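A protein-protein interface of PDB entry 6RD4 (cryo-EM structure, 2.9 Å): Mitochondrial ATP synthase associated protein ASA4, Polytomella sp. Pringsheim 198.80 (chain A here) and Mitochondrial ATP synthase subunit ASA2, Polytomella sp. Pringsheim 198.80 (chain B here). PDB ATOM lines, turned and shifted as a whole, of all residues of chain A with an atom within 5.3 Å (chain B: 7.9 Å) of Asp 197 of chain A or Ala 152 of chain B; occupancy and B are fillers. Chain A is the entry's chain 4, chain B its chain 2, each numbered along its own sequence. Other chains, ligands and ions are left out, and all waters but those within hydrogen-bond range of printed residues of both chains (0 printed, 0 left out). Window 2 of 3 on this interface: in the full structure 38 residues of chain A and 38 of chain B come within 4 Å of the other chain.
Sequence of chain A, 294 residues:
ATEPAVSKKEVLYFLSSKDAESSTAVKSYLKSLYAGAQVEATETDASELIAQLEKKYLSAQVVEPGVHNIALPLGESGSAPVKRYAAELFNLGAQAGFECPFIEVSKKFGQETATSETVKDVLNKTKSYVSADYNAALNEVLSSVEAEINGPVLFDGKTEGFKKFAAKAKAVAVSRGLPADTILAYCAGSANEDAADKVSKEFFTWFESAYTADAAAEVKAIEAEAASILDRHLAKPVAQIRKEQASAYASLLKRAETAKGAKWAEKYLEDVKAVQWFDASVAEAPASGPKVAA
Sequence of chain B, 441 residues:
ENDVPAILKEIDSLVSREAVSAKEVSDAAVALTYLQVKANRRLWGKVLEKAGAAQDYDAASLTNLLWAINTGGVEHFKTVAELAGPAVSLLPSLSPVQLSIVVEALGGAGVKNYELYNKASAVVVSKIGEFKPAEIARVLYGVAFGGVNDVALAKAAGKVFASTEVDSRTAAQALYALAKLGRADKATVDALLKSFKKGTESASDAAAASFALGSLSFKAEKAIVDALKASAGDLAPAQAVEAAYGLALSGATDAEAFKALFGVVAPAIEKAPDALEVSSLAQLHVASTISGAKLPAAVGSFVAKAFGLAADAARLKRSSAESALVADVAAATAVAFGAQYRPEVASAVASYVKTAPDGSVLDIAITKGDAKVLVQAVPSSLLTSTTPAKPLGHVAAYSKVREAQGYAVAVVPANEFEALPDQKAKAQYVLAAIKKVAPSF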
ATOM      1  N   ASN A 192      30.350 -28.771  -9.257  1.00  0.00           N
ATOM      2  CA  ASN A 192      29.962 -27.989  -8.096  1.00  0.00           C
ATOM      3  C   ASN A 192      28.451 -27.875  -8.006  1.00  0.00           C
ATOM      4  O   ASN A 192      27.749 -27.824  -9.016  1.00  0.00           O
ATOM      5  CB  ASN A 192      30.578 -26.599  -8.164  1.00  0.00           C
ATOM      6  CG  ASN A 192      30.528 -26.022  -9.554  1.00  0.00           C
ATOM      7  OD1 ASN A 192      30.065 -26.674 -10.484  1.00  0.00           O
ATOM      8  ND2 ASN A 192      31.015 -24.800  -9.710  1.00  0.00           N
ATOM      9  N   GLU A 193      27.951 -27.824  -6.776  1.00  0.00           N
ATOM     10  CA  GLU A 193      26.516 -27.714  -6.580  1.00  0.00           C
ATOM     11  C   GLU A 193      26.015 -26.293  -6.766  1.00  0.00           C
ATOM     12  O   GLU A 193      24.801 -26.084  -6.806  1.00  0.00           O
ATOM     13  CB  GLU A 193      26.125 -28.216  -5.193  1.00  0.00           C
ATOM     14  CG  GLU A 193      26.473 -27.276  -4.064  1.00  0.00           C
ATOM     15  CD  GLU A 193      26.029 -27.817  -2.722  1.00  0.00           C
ATOM     16  OE1 GLU A 193      26.864 -27.891  -1.797  1.00  0.00           O
ATOM     17  OE2 GLU A 193      24.842 -28.174  -2.594  1.00  0.00           O
ATOM     18  N   ASP A 194      26.909 -25.315  -6.869  1.00  0.00           N
ATOM     19  CA  ASP A 194      26.489 -23.943  -7.098  1.00  0.00           C
ATOM     20  C   ASP A 194      26.349 -23.601  -8.569  1.00  0.00           C
ATOM     21  O   ASP A 194      25.475 -22.810  -8.922  1.00  0.00           O
ATOM     22  CB  ASP A 194      27.462 -22.972  -6.437  1.00  0.00           C
ATOM     23  CG  ASP A 194      27.311 -22.943  -4.935  1.00  0.00           C
ATOM     24  OD1 ASP A 194      26.183 -23.168  -4.456  1.00  0.00           O
ATOM     25  OD2 ASP A 194      28.314 -22.701  -4.234  1.00  0.00           O
ATOM     26  N   ALA A 195      27.173 -24.160  -9.441  1.00  0.00           N
ATOM     27  CA  ALA A 195      26.992 -23.884 -10.857  1.00  0.00           C
ATOM     28  C   ALA A 195      25.947 -24.779 -11.494  1.00  0.00           C
ATOM     29  O   ALA A 195      25.460 -24.453 -12.579  1.00  0.00           O
ATOM     30  CB  ALA A 195      28.310 -24.036 -11.613  1.00  0.00           C
ATOM     31  N   ALA A 196      25.606 -25.901 -10.861  1.00  0.00           N
ATOM     32  CA  ALA A 196      24.476 -26.700 -11.308  1.00  0.00           C
ATOM     33  C   ALA A 196      23.160 -26.190 -10.751  1.00  0.00           C
ATOM     34  O   ALA A 196      22.102 -26.560 -11.264  1.00  0.00           O
ATOM     35  CB  ALA A 196      24.666 -28.163 -10.913  1.00  0.00           C
ATOM     36  N   ASP A 197      23.205 -25.344  -9.727  1.00  0.00           N
ATOM     37  CA  ASP A 197      22.001 -24.732  -9.190  1.00  0.00           C
ATOM     38  C   ASP A 197      21.475 -23.655 -10.121  1.00  0.00           C
ATOM     39  O   ASP A 197      20.265 -23.472 -10.245  1.00  0.00           O
ATOM     40  CB  ASP A 197      22.293 -24.144  -7.817  1.00  0.00           C
ATOM     41  CG  ASP A 197      21.101 -23.445  -7.211  1.00  0.00           C
ATOM     42  OD1 ASP A 197      20.288 -24.125  -6.555  1.00  0.00           O
ATOM     43  OD2 ASP A 197      20.980 -22.214  -7.371  1.00  0.00           O
ATOM     44  N   LYS A 198      22.367 -22.915 -10.764  1.00  0.00           N
ATOM     45  CA  LYS A 198      21.926 -21.876 -11.676  1.00  0.00           C
ATOM     46  C   LYS A 198      21.444 -22.431 -13.000  1.00  0.00           C
ATOM     47  O   LYS A 198      20.750 -21.718 -13.727  1.00  0.00           O
ATOM     48  CB  LYS A 198      23.041 -20.864 -11.948  1.00  0.00           C
ATOM     49  CG  LYS A 198      23.149 -19.713 -10.949  1.00  0.00           C
ATOM     50  CD  LYS A 198      23.815 -20.131  -9.660  1.00  0.00           C
ATOM     51  CE  LYS A 198      24.006 -18.972  -8.707  1.00  0.00           C
ATOM     52  NZ  LYS A 198      24.582 -19.412  -7.407  1.00  0.00           N
ATOM     53  N   VAL A 199      21.788 -23.669 -13.336  1.00  0.00           N
ATOM     54  CA  VAL A 199      21.280 -24.251 -14.567  1.00  0.00           C
ATOM     55  C   VAL A 199      19.992 -25.026 -14.306  1.00  0.00           C
ATOM     56  O   VAL A 199      19.199 -25.237 -15.227  1.00  0.00           O
ATOM     57  CB  VAL A 199      22.357 -25.127 -15.235  1.00  0.00           C
ATOM     58  CG1 VAL A 199      22.516 -26.456 -14.537  1.00  0.00           C
ATOM     59  CG2 VAL A 199      22.077 -25.310 -16.698  1.00  0.00           C
ATOM     60  N   SER A 200      19.736 -25.422 -13.057  1.00  0.00           N
ATOM     61  CA  SER A 200      18.454 -26.035 -12.754  1.00  0.00           C
ATOM     62  C   SER A 200      17.369 -24.988 -12.646  1.00  0.00           C
ATOM     63  O   SER A 200      16.225 -25.251 -13.012  1.00  0.00           O
ATOM     64  CB  SER A 200      18.512 -26.827 -11.457  1.00  0.00           C
ATOM     65  OG  SER A 200      18.497 -25.951 -10.355  1.00  0.00           O
ATOM     66  N   LYS A 201      17.709 -23.793 -12.179  1.00  0.00           N
ATOM     67  CA  LYS A 201      16.745 -22.710 -12.111  1.00  0.00           C
ATOM     68  C   LYS A 201      16.397 -22.128 -13.466  1.00  0.00           C
ATOM     69  O   LYS A 201      15.436 -21.365 -13.553  1.00  0.00           O
ATOM     70  CB  LYS A 201      17.261 -21.587 -11.227  1.00  0.00           C
ATOM     71  CG  LYS A 201      17.225 -21.890  -9.757  1.00  0.00           C
ATOM     72  CD  LYS A 201      18.048 -20.889  -9.004  1.00  0.00           C
ATOM     73  CE  LYS A 201      17.603 -19.475  -9.292  1.00  0.00           C
ATOM     74  NZ  LYS A 201      16.246 -19.210  -8.772  1.00  0.00           N
ATOM     75  N   ASN B 118      11.147 -19.216  -7.833  1.00  0.00           N
ATOM     76  CA  ASN B 118      12.332 -18.602  -8.417  1.00  0.00           C
ATOM     77  C   ASN B 118      12.353 -17.113  -8.139  1.00  0.00           C
ATOM     78  O   ASN B 118      13.388 -16.559  -7.762  1.00  0.00           O
ATOM     79  CB  ASN B 118      12.402 -18.849  -9.918  1.00  0.00           C
ATOM     80  CG  ASN B 118      12.908 -20.224 -10.256  1.00  0.00           C
ATOM     81  OD1 ASN B 118      12.886 -20.640 -11.409  1.00  0.00           O
ATOM     82  ND2 ASN B 118      13.350 -20.951  -9.246  1.00  0.00           N
ATOM     83  N   SER B 121      12.714 -16.606  -4.206  1.00  0.00           N
ATOM     84  CA  SER B 121      14.046 -16.781  -3.644  1.00  0.00           C
ATOM     85  C   SER B 121      15.010 -15.726  -4.147  1.00  0.00           C
ATOM     86  O   SER B 121      15.928 -15.341  -3.420  1.00  0.00           O
ATOM     87  CB  SER B 121      14.610 -18.149  -3.982  1.00  0.00           C
ATOM     88  OG  SER B 121      14.974 -18.193  -5.345  1.00  0.00           O
ATOM     89  N   VAL B 124      14.568 -12.929  -1.862  1.00  0.00           N
ATOM     90  CA  VAL B 124      15.069 -13.105  -0.502  1.00  0.00           C
ATOM     91  C   VAL B 124      16.583 -13.253  -0.451  1.00  0.00           C
ATOM     92  O   VAL B 124      17.162 -13.267   0.642  1.00  0.00           O
ATOM     93  CB  VAL B 124      14.342 -14.300   0.141  1.00  0.00           C
ATOM     94  CG1 VAL B 124      14.997 -15.585  -0.233  1.00  0.00           C
ATOM     95  CG2 VAL B 124      14.229 -14.143   1.629  1.00  0.00           C
ATOM     96  N   VAL B 125      17.255 -13.357  -1.598  1.00  0.00           N
ATOM     97  CA  VAL B 125      18.705 -13.204  -1.625  1.00  0.00           C
ATOM     98  C   VAL B 125      19.142 -11.836  -2.146  1.00  0.00           C
ATOM     99  O   VAL B 125      20.290 -11.438  -1.907  1.00  0.00           O
ATOM    100  CB  VAL B 125      19.385 -14.328  -2.437  1.00  0.00           C
ATOM    101  CG1 VAL B 125      18.953 -15.677  -1.924  1.00  0.00           C
ATOM    102  CG2 VAL B 125      19.092 -14.198  -3.906  1.00  0.00           C
ATOM    103  N   ILE B 128      18.842  -9.852   1.603  1.00  0.00           N
ATOM    104  CA  ILE B 128      18.975 -10.896   2.605  1.00  0.00           C
ATOM    105  C   ILE B 128      18.969 -10.308   4.015  1.00  0.00           C
ATOM    106  O   ILE B 128      18.434 -10.927   4.941  1.00  0.00           O
ATOM    107  CB  ILE B 128      20.227 -11.750   2.321  1.00  0.00           C
ATOM    108  CG1 ILE B 128      20.353 -12.906   3.314  1.00  0.00           C
ATOM    109  CG2 ILE B 128      21.489 -10.899   2.258  1.00  0.00           C
ATOM    110  CD1 ILE B 128      19.172 -13.831   3.315  1.00  0.00           C
ATOM    111  N   LEU B 140      12.417 -20.859   3.204  1.00  0.00           N
ATOM    112  CA  LEU B 140      13.168 -22.086   2.979  1.00  0.00           C
ATOM    113  C   LEU B 140      12.281 -23.310   3.119  1.00  0.00           C
ATOM    114  O   LEU B 140      12.470 -24.296   2.412  1.00  0.00           O
ATOM    115  CB  LEU B 140      14.342 -22.161   3.947  1.00  0.00           C
ATOM    116  CG  LEU B 140      15.340 -23.294   3.783  1.00  0.00           C
ATOM    117  CD1 LEU B 140      16.017 -23.189   2.452  1.00  0.00           C
ATOM    118  CD2 LEU B 140      16.338 -23.229   4.895  1.00  0.00           C
ATOM    119  N   VAL B 148      11.410 -27.345  -5.231  1.00  0.00           N
ATOM    120  CA  VAL B 148      12.543 -26.644  -5.814  1.00  0.00           C
ATOM    121  C   VAL B 148      13.761 -26.954  -4.967  1.00  0.00           C
ATOM    122  O   VAL B 148      13.773 -26.681  -3.766  1.00  0.00           O
ATOM    123  CB  VAL B 148      12.295 -25.133  -5.874  1.00  0.00           C
ATOM    124  CG1 VAL B 148      13.478 -24.435  -6.465  1.00  0.00           C
ATOM    125  CG2 VAL B 148      11.080 -24.832  -6.667  1.00  0.00           C
ATOM    126  N   ASN B 149      14.793 -27.517  -5.577  1.00  0.00           N
ATOM    127  CA  ASN B 149      16.023 -27.793  -4.841  1.00  0.00           C
ATOM    128  C   ASN B 149      16.977 -26.608  -4.956  1.00  0.00           C
ATOM    129  O   ASN B 149      18.067 -26.694  -5.509  1.00  0.00           O
ATOM    130  CB  ASN B 149      16.672 -29.073  -5.339  1.00  0.00           C
ATOM    131  CG  ASN B 149      17.574 -29.694  -4.306  1.00  0.00           C
ATOM    132  OD1 ASN B 149      18.738 -29.329  -4.185  1.00  0.00           O
ATOM    133  ND2 ASN B 149      17.038 -30.638  -3.547  1.00  0.00           N
ATOM    134  N   ASP B 150      16.529 -25.479  -4.421  1.00  0.00           N
ATOM    135  CA  ASP B 150      17.287 -24.241  -4.507  1.00  0.00           C
ATOM    136  C   ASP B 150      18.341 -24.256  -3.421  1.00  0.00           C
ATOM    137  O   ASP B 150      18.043 -23.960  -2.260  1.00  0.00           O
ATOM    138  CB  ASP B 150      16.375 -23.033  -4.347  1.00  0.00           C
ATOM    139  CG  ASP B 150      16.855 -21.847  -5.131  1.00  0.00           C
ATOM    140  OD1 ASP B 150      17.744 -22.024  -5.979  1.00  0.00           O
ATOM    141  OD2 ASP B 150      16.357 -20.736  -4.905  1.00  0.00           O
ATOM    142  N   VAL B 151      19.574 -24.605  -3.787  1.00  0.00           N
ATOM    143  CA  VAL B 151      20.654 -24.577  -2.811  1.00  0.00           C
ATOM    144  C   VAL B 151      21.301 -23.212  -2.723  1.00  0.00           C
ATOM    145  O   VAL B 151      22.116 -22.989  -1.821  1.00  0.00           O
ATOM    146  CB  VAL B 151      21.738 -25.626  -3.117  1.00  0.00           C
ATOM    147  CG1 VAL B 151      21.115 -27.000  -3.247  1.00  0.00           C
ATOM    148  CG2 VAL B 151      22.499 -25.253  -4.347  1.00  0.00           C
ATOM    149  N   ALA B 152      20.972 -22.292  -3.629  1.00  0.00           N
ATOM    150  CA  ALA B 152      21.435 -20.920  -3.478  1.00  0.00           C
ATOM    151  C   ALA B 152      20.788 -20.260  -2.275  1.00  0.00           C
ATOM    152  O   ALA B 152      21.434 -19.494  -1.558  1.00  0.00           O
ATOM    153  CB  ALA B 152      21.141 -20.122  -4.742  1.00  0.00           C
ATOM    154  N   LEU B 153      19.517 -20.558  -2.029  1.00  0.00           N
ATOM    155  CA  LEU B 153      18.854 -20.043  -0.844  1.00  0.00           C
ATOM    156  C   LEU B 153      19.303 -20.782   0.405  1.00  0.00           C
ATOM    157  O   LEU B 153      19.415 -20.174   1.472  1.00  0.00           O
ATOM    158  CB  LEU B 153      17.341 -20.137  -1.022  1.00  0.00           C
ATOM    159  CG  LEU B 153      16.416 -20.171   0.192  1.00  0.00           C
ATOM    160  CD1 LEU B 153      16.380 -18.834   0.862  1.00  0.00           C
ATOM    161  CD2 LEU B 153      15.039 -20.594  -0.219  1.00  0.00           C
ATOM    162  N   ALA B 154      19.584 -22.079   0.291  1.00  0.00           N
ATOM    163  CA  ALA B 154      19.963 -22.863   1.461  1.00  0.00           C
ATOM    164  C   ALA B 154      21.351 -22.494   1.958  1.00  0.00           C
ATOM    165  O   ALA B 154      21.677 -22.731   3.124  1.00  0.00           O
ATOM    166  CB  ALA B 154      19.893 -24.349   1.138  1.00  0.00           C
ATOM    167  N   LYS B 155      22.180 -21.922   1.090  1.00  0.00           N
ATOM    168  CA  LYS B 155      23.439 -21.352   1.535  1.00  0.00           C
ATOM    169  C   LYS B 155      23.227 -19.987   2.168  1.00  0.00           C
ATOM    170  O   LYS B 155      23.765 -19.712   3.244  1.00  0.00           O
ATOM    171  CB  LYS B 155      24.401 -21.261   0.358  1.00  0.00           C
ATOM    172  CG  LYS B 155      24.868 -22.612  -0.088  1.00  0.00           C
ATOM    173  CD  LYS B 155      25.988 -22.527  -1.078  1.00  0.00           C
ATOM    174  CE  LYS B 155      26.601 -23.897  -1.257  1.00  0.00           C
ATOM    175  NZ  LYS B 155      27.925 -23.828  -1.914  1.00  0.00           N
ATOM    176  N   ALA B 156      22.421 -19.136   1.530  1.00  0.00           N
ATOM    177  CA  ALA B 156      22.158 -17.808   2.068  1.00  0.00           C
ATOM    178  C   ALA B 156      21.361 -17.867   3.359  1.00  0.00           C
ATOM    179  O   ALA B 156      21.484 -16.977   4.201  1.00  0.00           O
ATOM    180  CB  ALA B 156      21.424 -16.962   1.035  1.00  0.00           C
ATOM    181  N   ALA B 157      20.546 -18.899   3.540  1.00  0.00           N
ATOM    182  CA  ALA B 157      19.917 -19.098   4.837  1.00  0.00           C
ATOM    183  C   ALA B 157      20.909 -19.636   5.847  1.00  0.00           C
ATOM    184  O   ALA B 157      20.804 -19.332   7.034  1.00  0.00           O
ATOM    185  CB  ALA B 157      18.728 -20.046   4.717  1.00  0.00           C
ATOM    186  N   GLY B 158      21.884 -20.424   5.392  1.00  0.00           N
ATOM    187  CA  GLY B 158      22.881 -20.957   6.301  1.00  0.00           C
ATOM    188  C   GLY B 158      23.841 -19.910   6.828  1.00  0.00           C
ATOM    189  O   GLY B 158      24.339 -20.031   7.952  1.00  0.00           O
ATOM    190  N   LYS B 159      24.105 -18.870   6.040  1.00  0.00           N
ATOM    191  CA  LYS B 159      24.916 -17.766   6.531  1.00  0.00           C
ATOM    192  C   LYS B 159      24.159 -16.918   7.541  1.00  0.00           C
ATOM    193  O   LYS B 159      24.776 -16.311   8.420  1.00  0.00           O
ATOM    194  CB  LYS B 159      25.391 -16.917   5.361  1.00  0.00           C
ATOM    195  CG  LYS B 159      26.427 -17.621   4.526  1.00  0.00           C
ATOM    196  CD  LYS B 159      26.746 -16.852   3.271  1.00  0.00           C
ATOM    197  CE  LYS B 159      27.824 -17.563   2.480  1.00  0.00           C
ATOM    198  NZ  LYS B 159      27.493 -18.996   2.256  1.00  0.00           N
ATOM    199  N   LEU B 181      15.243 -31.231   1.542  1.00  0.00           N
ATOM    200  CA  LEU B 181      16.276 -31.011   0.545  1.00  0.00           C
ATOM    201  C   LEU B 181      17.390 -32.038   0.645  1.00  0.00           C
ATOM    202  O   LEU B 181      18.093 -32.262  -0.344  1.00  0.00           O
ATOM    203  CB  LEU B 181      16.860 -29.613   0.682  1.00  0.00           C
ATOM    204  CG  LEU B 181      15.972 -28.444   0.303  1.00  0.00           C
ATOM    205  CD1 LEU B 181      16.759 -27.180   0.333  1.00  0.00           C
ATOM    206  CD2 LEU B 181      15.420 -28.651  -1.057  1.00  0.00           C
ATOM    207  N   ARG B 183      20.219 -32.182   2.875  1.00  0.00           N
ATOM    208  CA  ARG B 183      21.462 -31.439   2.798  1.00  0.00           C
ATOM    209  C   ARG B 183      22.468 -31.843   3.860  1.00  0.00           C
ATOM    210  O   ARG B 183      23.629 -32.097   3.523  1.00  0.00           O
ATOM    211  CB  ARG B 183      21.175 -29.945   2.863  1.00  0.00           C
ATOM    212  CG  ARG B 183      20.702 -29.439   1.540  1.00  0.00           C
ATOM    213  CD  ARG B 183      20.890 -27.962   1.431  1.00  0.00           C
ATOM    214  NE  ARG B 183      22.271 -27.575   1.649  1.00  0.00           N
ATOM    215  CZ  ARG B 183      23.197 -27.564   0.701  1.00  0.00           C
ATOM    216  NH1 ARG B 183      22.891 -27.929  -0.528  1.00  0.00           N
ATOM    217  NH2 ARG B 183      24.432 -27.187   0.982  1.00  0.00           N
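The side-chain hydroxyl (OG) of Ser 121 of chain B is in hydrogen-bond range of the side-chain carboxylate (OD2) of Asp 150 of chain B, at 2.9 Å. O of Asp 197 of chain A lies within hydrogen-bond range of OG of Ser 200 of chain A, at 3.0 Å. The side-chain hydroxyl of Ser 121 of chain B lies within hydrogen-bond range of the backbone carbonyl oxygen of Asn 118 of chain B.
Among the printed residues, merely in contact across the chains: Glu 193 of chain A with Val 151 of chain B (3.5 Å), Asp 197 of chain A with Asn 149 of chain B (3.6 Å), Asp 197 of chain A with Ala 152 of chain B (3.4 Å), Lys 201 of chain A with Ser 121 of chain B (3.8 Å) and Lys 201 of chain A with Asp 150 of chain B (3.2 Å).
OD2 of Asp 194 of chain A is in salt-bridge range of NZ of Lys 155 of chain B (2.6 Å). The side-chain carboxylate (OD1) of Asp 197 of chain A lies close to the side-chain carboxylate (OD1) of Asp 150 of chain B (3.3 Å). NH1 of Arg 183 of chain B lies within salt-bridge range of OE2 of Glu 193 of chain A (2.9 Å). The side-chain amide oxygen (OD1) of Asn 118 of chain B lies close to the backbone carbonyl oxygen (O) of Lys 201 of chain A, at 3.4 Å. N of Val 151 of chain B lies within hydrogen-bond range of OD1 of Asp 197 of chain A (2.9 Å).
Printed residues of chain B within 4 Å of Glu 193 of chain A: Val 151 (3.5 Å) and Arg 183 (2.9 Å). Printed residues of chain B within 4 Å of Asp 194 of chain A: Lys 155 (2.6 Å). Of chain B, only Asn 149, Asp 150, Val 151 and Ala 152 come within 4 Å of Asp 197 of chain A. Val 199 of chain A touches none of the printed residues of chain B. Of the printed residues of chain B, Lys 201 of chain A touches Asn 118 (3.4 Å), Ser 121 (3.8 Å) and Asp 150 (3.2 Å). Printed residues of chain A within 4 Å of Asn 118 of chain B: Lys 201. Of the printed residues of chain A, Asp 150 of chain B touches Asp 197 and Lys 201. Of chain A, only Asp 197 comes within 4 Å of Ala 152 of chain B. Ala 154 of chain B touches none of the printed residues of chain A.
Of the 20 printed residues of chain B, 8 touch a printed residue of chain A. Hydrophobic or aromatic side chains of chain B that line the printed part of chain A: Val 151 and Ala 152. Of the 10 printed residues of chain A, 4 touch a printed residue of chain B. Among the printed residues, 10 pairs touch across the chains.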
